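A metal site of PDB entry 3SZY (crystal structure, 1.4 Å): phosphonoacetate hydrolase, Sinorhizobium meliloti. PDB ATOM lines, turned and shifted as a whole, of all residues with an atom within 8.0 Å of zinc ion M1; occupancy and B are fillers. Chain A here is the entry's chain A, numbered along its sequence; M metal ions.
The side-chain amide oxygen (OE1) of Gln 217 lies close to the backbone carbonyl oxygen (O) of Asp 214.
ND1 of His 380 lies close to ND1 of His 254 (3.5 Å).
ND1 of His 380 is in hydrogen-bond range of O of Ser 69 (2.8 Å).
A ring nitrogen (ND1) of His 218 sits at hydrogen-bond distance from the backbone carbonyl oxygen (O) of Arg 378, 2.8 Å away.
The nearest printed residue that does not touch zinc ion M1 is Thr 71 (4.3 Å).
Zinc ion M1 is bound by OD2 of Asp 214.
NE2 of His 380 is bound to zinc ion M1, 2.1 Å away.
NE2 of His 218 binds zinc ion M1 (2.1 Å).
Zinc ion M1 has three donor atoms within binding distance.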
ATOM      1  N   ASP A  32      19.682  10.804 -17.274  1.00  0.00           N
ATOM      2  CA  ASP A  32      18.829  11.905 -16.853  1.00  0.00           C
ATOM      3  C   ASP A  32      17.619  12.079 -17.782  1.00  0.00           C
ATOM      4  O   ASP A  32      17.784  12.173 -19.001  1.00  0.00           O
ATOM      5  CB  ASP A  32      19.665  13.179 -16.799  1.00  0.00           C
ATOM      6  CG  ASP A  32      19.054  14.230 -15.920  1.00  0.00           C
ATOM      7  OD1 ASP A  32      17.807  14.349 -15.892  1.00  0.00           O
ATOM      8  OD2 ASP A  32      19.813  14.962 -15.255  1.00  0.00           O
ATOM      9  N   GLY A  33      16.429  12.114 -17.199  1.00  0.00           N
ATOM     10  CA  GLY A  33      15.194  12.339 -17.952  1.00  0.00           C
ATOM     11  C   GLY A  33      14.816  11.220 -18.905  1.00  0.00           C
ATOM     12  O   GLY A  33      13.990  11.424 -19.793  1.00  0.00           O
ATOM     13  N   SER A  69       9.827  14.417  -8.904  1.00  0.00           N
ATOM     14  CA  SER A  69      10.672  13.776  -9.913  1.00  0.00           C
ATOM     15  C   SER A  69      11.604  14.818 -10.547  1.00  0.00           C
ATOM     16  O   SER A  69      11.505  15.118 -11.736  1.00  0.00           O
ATOM     17  CB  SER A  69       9.823  12.988 -10.933  1.00  0.00           C
ATOM     18  OG  SER A  69       8.809  13.769 -11.528  1.00  0.00           O
ATOM     19  N   PHE A  70      12.496  15.331  -9.705  1.00  0.00           N
ATOM     20  CA  PHE A  70      13.484  16.362 -10.026  1.00  0.00           C
ATOM     21  C   PHE A  70      14.885  15.738 -10.033  1.00  0.00           C
ATOM     22  O   PHE A  70      15.118  14.687  -9.418  1.00  0.00           O
ATOM     23  CB  PHE A  70      13.512  17.462  -8.949  1.00  0.00           C
ATOM     24  CG  PHE A  70      12.281  18.334  -8.878  1.00  0.00           C
ATOM     25  CD1 PHE A  70      11.392  18.480  -9.948  1.00  0.00           C
ATOM     26  CD2 PHE A  70      12.056  19.087  -7.724  1.00  0.00           C
ATOM     27  CE1 PHE A  70      10.279  19.326  -9.830  1.00  0.00           C
ATOM     28  CE2 PHE A  70      10.954  19.925  -7.606  1.00  0.00           C
ATOM     29  CZ  PHE A  70      10.067  20.046  -8.655  1.00  0.00           C
ATOM     30  N   THR A  71      15.821  16.424 -10.688  1.00  0.00           N
ATOM     31  CA  THR A  71      17.193  15.932 -10.864  1.00  0.00           C
ATOM     32  C   THR A  71      17.977  15.731  -9.566  1.00  0.00           C
ATOM     33  O   THR A  71      18.437  14.624  -9.289  1.00  0.00           O
ATOM     34  CB  THR A  71      17.967  16.860 -11.832  1.00  0.00           C
ATOM     35  OG1 THR A  71      17.316  16.831 -13.117  1.00  0.00           O
ATOM     36  CG2 THR A  71      19.408  16.426 -11.995  1.00  0.00           C
ATOM     37  N   THR A 213      22.899  14.820 -18.095  1.00  0.00           N
ATOM     38  CA  THR A 213      21.868  15.867 -18.005  1.00  0.00           C
ATOM     39  C   THR A 213      20.701  15.532 -18.925  1.00  0.00           C
ATOM     40  O   THR A 213      20.848  14.713 -19.842  1.00  0.00           O
ATOM     41  CB  THR A 213      22.350  17.306 -18.359  1.00  0.00           C
ATOM     42  OG1 THR A 213      22.364  17.484 -19.784  1.00  0.00           O
ATOM     43  CG2 THR A 213      23.700  17.623 -17.759  1.00  0.00           C
ATOM     44  N   ASP A 214      19.571  16.172 -18.652  1.00  0.00           N
ATOM     45  CA  ASP A 214      18.330  15.981 -19.399  1.00  0.00           C
ATOM     46  C   ASP A 214      18.156  16.980 -20.555  1.00  0.00           C
ATOM     47  O   ASP A 214      17.026  17.232 -20.991  1.00  0.00           O
ATOM     48  CB  ASP A 214      17.100  15.984 -18.448  1.00  0.00           C
ATOM     49  CG  ASP A 214      16.963  17.281 -17.619  1.00  0.00           C
ATOM     50  OD1 ASP A 214      17.835  18.159 -17.735  1.00  0.00           O
ATOM     51  OD2 ASP A 214      15.965  17.436 -16.847  1.00  0.00           O
ATOM     52  N   TYR A 215      19.256  17.536 -21.056  1.00  0.00           N
ATOM     53  CA  TYR A 215      19.216  18.535 -22.136  1.00  0.00           C
ATOM     54  C   TYR A 215      18.461  18.053 -23.373  1.00  0.00           C
ATOM     55  O   TYR A 215      17.517  18.716 -23.827  1.00  0.00           O
ATOM     56  CB  TYR A 215      20.627  18.988 -22.533  1.00  0.00           C
ATOM     57  CG  TYR A 215      20.653  19.828 -23.788  1.00  0.00           C
ATOM     58  CD1 TYR A 215      20.285  21.172 -23.763  1.00  0.00           C
ATOM     59  CD2 TYR A 215      21.007  19.272 -25.024  1.00  0.00           C
ATOM     60  CE1 TYR A 215      20.300  21.952 -24.924  1.00  0.00           C
ATOM     61  CE2 TYR A 215      21.013  20.038 -26.188  1.00  0.00           C
ATOM     62  CZ  TYR A 215      20.672  21.371 -26.121  1.00  0.00           C
ATOM     63  OH  TYR A 215      20.672  22.138 -27.273  1.00  0.00           O
ATOM     64  N   GLN A 217      16.529  15.516 -23.672  1.00  0.00           N
ATOM     65  CA  GLN A 217      15.211  14.999 -23.318  1.00  0.00           C
ATOM     66  C   GLN A 217      14.163  16.098 -23.122  1.00  0.00           C
ATOM     67  O   GLN A 217      12.993  15.918 -23.470  1.00  0.00           O
ATOM     68  CB  GLN A 217      15.331  14.087 -22.083  1.00  0.00           C
ATOM     69  CG  GLN A 217      16.200  12.832 -22.290  1.00  0.00           C
ATOM     70  CD  GLN A 217      17.692  13.115 -22.449  1.00  0.00           C
ATOM     71  OE1 GLN A 217      18.220  14.109 -21.942  1.00  0.00           O
ATOM     72  NE2 GLN A 217      18.395  12.236 -23.156  1.00  0.00           N
ATOM     73  N   HIS A 218      14.582  17.252 -22.595  1.00  0.00           N
ATOM     74  CA  HIS A 218      13.708  18.435 -22.536  1.00  0.00           C
ATOM     75  C   HIS A 218      13.370  18.955 -23.930  1.00  0.00           C
ATOM     76  O   HIS A 218      12.322  19.564 -24.122  1.00  0.00           O
ATOM     77  CB  HIS A 218      14.346  19.572 -21.726  1.00  0.00           C
ATOM     78  CG  HIS A 218      14.117  19.490 -20.250  1.00  0.00           C
ATOM     79  ND1 HIS A 218      12.921  19.814 -19.651  1.00  0.00           N
ATOM     80  CD2 HIS A 218      14.966  19.159 -19.238  1.00  0.00           C
ATOM     81  CE1 HIS A 218      13.024  19.667 -18.337  1.00  0.00           C
ATOM     82  NE2 HIS A 218      14.253  19.269 -18.068  1.00  0.00           N
ATOM     83  N   ASP A 253      16.970   9.337 -13.115  1.00  0.00           N
ATOM     84  CA  ASP A 253      16.500  10.168 -12.005  1.00  0.00           C
ATOM     85  C   ASP A 253      14.994  10.447 -12.085  1.00  0.00           C
ATOM     86  O   ASP A 253      14.334  10.537 -11.054  1.00  0.00           O
ATOM     87  CB  ASP A 253      17.320  11.468 -11.891  1.00  0.00           C
ATOM     88  CG  ASP A 253      17.388  12.271 -13.198  1.00  0.00           C
ATOM     89  OD1 ASP A 253      16.929  11.793 -14.259  1.00  0.00           O
ATOM     90  OD2 ASP A 253      17.920  13.402 -13.137  1.00  0.00           O
ATOM     91  N   HIS A 254      14.472  10.546 -13.300  1.00  0.00           N
ATOM     92  CA  HIS A 254      13.058  10.803 -13.562  1.00  0.00           C
ATOM     93  C   HIS A 254      12.820  10.641 -15.058  1.00  0.00           C
ATOM     94  O   HIS A 254      13.774  10.591 -15.839  1.00  0.00           O
ATOM     95  CB  HIS A 254      12.659  12.223 -13.148  1.00  0.00           C
ATOM     96  CG  HIS A 254      13.559  13.279 -13.712  1.00  0.00           C
ATOM     97  ND1 HIS A 254      13.460  13.716 -15.013  1.00  0.00           N
ATOM     98  CD2 HIS A 254      14.608  13.945 -13.176  1.00  0.00           C
ATOM     99  CE1 HIS A 254      14.395  14.619 -15.245  1.00  0.00           C
ATOM    100  NE2 HIS A 254      15.109  14.768 -14.150  1.00  0.00           N
ATOM    101  N   GLY A 255      11.548  10.594 -15.444  1.00  0.00           N
ATOM    102  CA  GLY A 255      11.154  10.567 -16.854  1.00  0.00           C
ATOM    103  C   GLY A 255      10.957  11.960 -17.430  1.00  0.00           C
ATOM    104  O   GLY A 255      11.551  12.940 -16.957  1.00  0.00           O
ATOM    105  N   MET A 256      10.126  12.049 -18.459  1.00  0.00           N
ATOM    106  CA  MET A 256       9.912  13.297 -19.193  1.00  0.00           C
ATOM    107  C   MET A 256       8.599  13.166 -19.958  1.00  0.00           C
ATOM    108  O   MET A 256       8.338  12.122 -20.561  1.00  0.00           O
ATOM    109  CB  MET A 256      11.066  13.550 -20.164  1.00  0.00           C
ATOM    110  CG  MET A 256      11.104  14.960 -20.765  1.00  0.00           C
ATOM    111  SD  MET A 256      11.618  16.240 -19.614  1.00  0.00           S
ATOM    112  CE  MET A 256      13.328  15.773 -19.323  1.00  0.00           C
ATOM    113  N   ILE A 290      12.122  22.896  -9.108  1.00  0.00           N
ATOM    114  CA  ILE A 290      12.694  22.152 -10.248  1.00  0.00           C
ATOM    115  C   ILE A 290      14.054  22.712 -10.675  1.00  0.00           C
ATOM    116  O   ILE A 290      14.908  21.965 -11.153  1.00  0.00           O
ATOM    117  CB  ILE A 290      11.728  22.081 -11.475  1.00  0.00           C
ATOM    118  CG1 ILE A 290      12.272  21.088 -12.515  1.00  0.00           C
ATOM    119  CG2 ILE A 290      11.466  23.478 -12.080  1.00  0.00           C
ATOM    120  CD1 ILE A 290      11.278  20.672 -13.571  1.00  0.00           C
ATOM    121  N   THR A 291      14.235  24.013 -10.513  1.00  0.00           N
ATOM    122  CA  THR A 291      15.502  24.662 -10.852  1.00  0.00           C
ATOM    123  C   THR A 291      15.799  25.782  -9.855  1.00  0.00           C
ATOM    124  O   THR A 291      15.088  25.953  -8.865  1.00  0.00           O
ATOM    125  CB  THR A 291      15.501  25.181 -12.324  1.00  0.00           C
ATOM    126  OG1 THR A 291      16.829  25.552 -12.698  1.00  0.00           O
ATOM    127  CG2 THR A 291      14.569  26.381 -12.490  1.00  0.00           C
ATOM    128  N   GLY A 299      12.455  27.046 -18.158  1.00  0.00           N
ATOM    129  CA  GLY A 299      13.188  26.020 -17.419  1.00  0.00           C
ATOM    130  C   GLY A 299      12.711  25.873 -15.983  1.00  0.00           C
ATOM    131  O   GLY A 299      12.948  24.854 -15.338  1.00  0.00           O
ATOM    132  N   LEU A 301       9.657  25.643 -15.216  1.00  0.00           N
ATOM    133  CA  LEU A 301       8.349  25.004 -15.304  1.00  0.00           C
ATOM    134  C   LEU A 301       8.419  23.497 -15.159  1.00  0.00           C
ATOM    135  O   LEU A 301       8.924  22.786 -16.038  1.00  0.00           O
ATOM    136  CB  LEU A 301       7.636  25.402 -16.603  1.00  0.00           C
ATOM    137  CG  LEU A 301       7.337  26.889 -16.800  1.00  0.00           C
ATOM    138  CD1 LEU A 301       6.800  27.142 -18.198  1.00  0.00           C
ATOM    139  CD2 LEU A 301       6.363  27.413 -15.730  1.00  0.00           C
ATOM    140  N   ARG A 378       8.703  20.425 -22.728  1.00  0.00           N
ATOM    141  CA  ARG A 378       8.724  19.097 -22.131  1.00  0.00           C
ATOM    142  C   ARG A 378       9.332  19.256 -20.744  1.00  0.00           C
ATOM    143  O   ARG A 378      10.281  20.025 -20.568  1.00  0.00           O
ATOM    144  CB  ARG A 378       9.571  18.132 -22.963  1.00  0.00           C
ATOM    145  CG  ARG A 378       9.090  17.938 -24.403  1.00  0.00           C
ATOM    146  CD  ARG A 378      10.045  17.067 -25.214  1.00  0.00           C
ATOM    147  NE  ARG A 378      10.339  15.789 -24.578  1.00  0.00           N
ATOM    148  CZ  ARG A 378       9.479  14.768 -24.473  1.00  0.00           C
ATOM    149  NH1 ARG A 378       8.259  14.861 -24.976  1.00  0.00           N
ATOM    150  NH2 ARG A 378       9.851  13.658 -23.860  1.00  0.00           N
ATOM    151  N   SER A 379       8.785  18.560 -19.743  1.00  0.00           N
ATOM    152  CA  SER A 379       9.335  18.667 -18.397  1.00  0.00           C
ATOM    153  C   SER A 379       8.979  17.488 -17.504  1.00  0.00           C
ATOM    154  O   SER A 379       8.493  16.454 -17.974  1.00  0.00           O
ATOM    155  CB  SER A 379       8.951  19.997 -17.738  1.00  0.00           C
ATOM    156  OG  SER A 379       9.851  20.328 -16.690  1.00  0.00           O
ATOM    157  N   HIS A 380       9.221  17.663 -16.204  1.00  0.00           N
ATOM    158  CA  HIS A 380       9.120  16.586 -15.233  1.00  0.00           C
ATOM    159  C   HIS A 380       8.794  17.170 -13.871  1.00  0.00           C
ATOM    160  O   HIS A 380       8.503  18.368 -13.762  1.00  0.00           O
ATOM    161  CB  HIS A 380      10.429  15.771 -15.203  1.00  0.00           C
ATOM    162  CG  HIS A 380      11.666  16.602 -15.063  1.00  0.00           C
ATOM    163  ND1 HIS A 380      12.302  16.799 -13.855  1.00  0.00           N
ATOM    164  CD2 HIS A 380      12.380  17.298 -15.986  1.00  0.00           C
ATOM    165  CE1 HIS A 380      13.353  17.578 -14.034  1.00  0.00           C
ATOM    166  NE2 HIS A 380      13.422  17.895 -15.319  1.00  0.00           N
ATOM    167  N   GLY A 381       8.811  16.338 -12.831  1.00  0.00           N
ATOM    168  CA  GLY A 381       8.510  16.776 -11.471  1.00  0.00           C
ATOM    169  C   GLY A 381       7.312  16.070 -10.871  1.00  0.00           C
ATOM    170  O   GLY A 381       7.234  15.902  -9.656  1.00  0.00           O
HETATM  171 ZN    ZN M   1      15.076  18.981 -16.109  1.00  0.00          ZN
HETATM  172 ZN    ZN M   2      17.048  15.211 -14.361  1.00  0.00          ZN
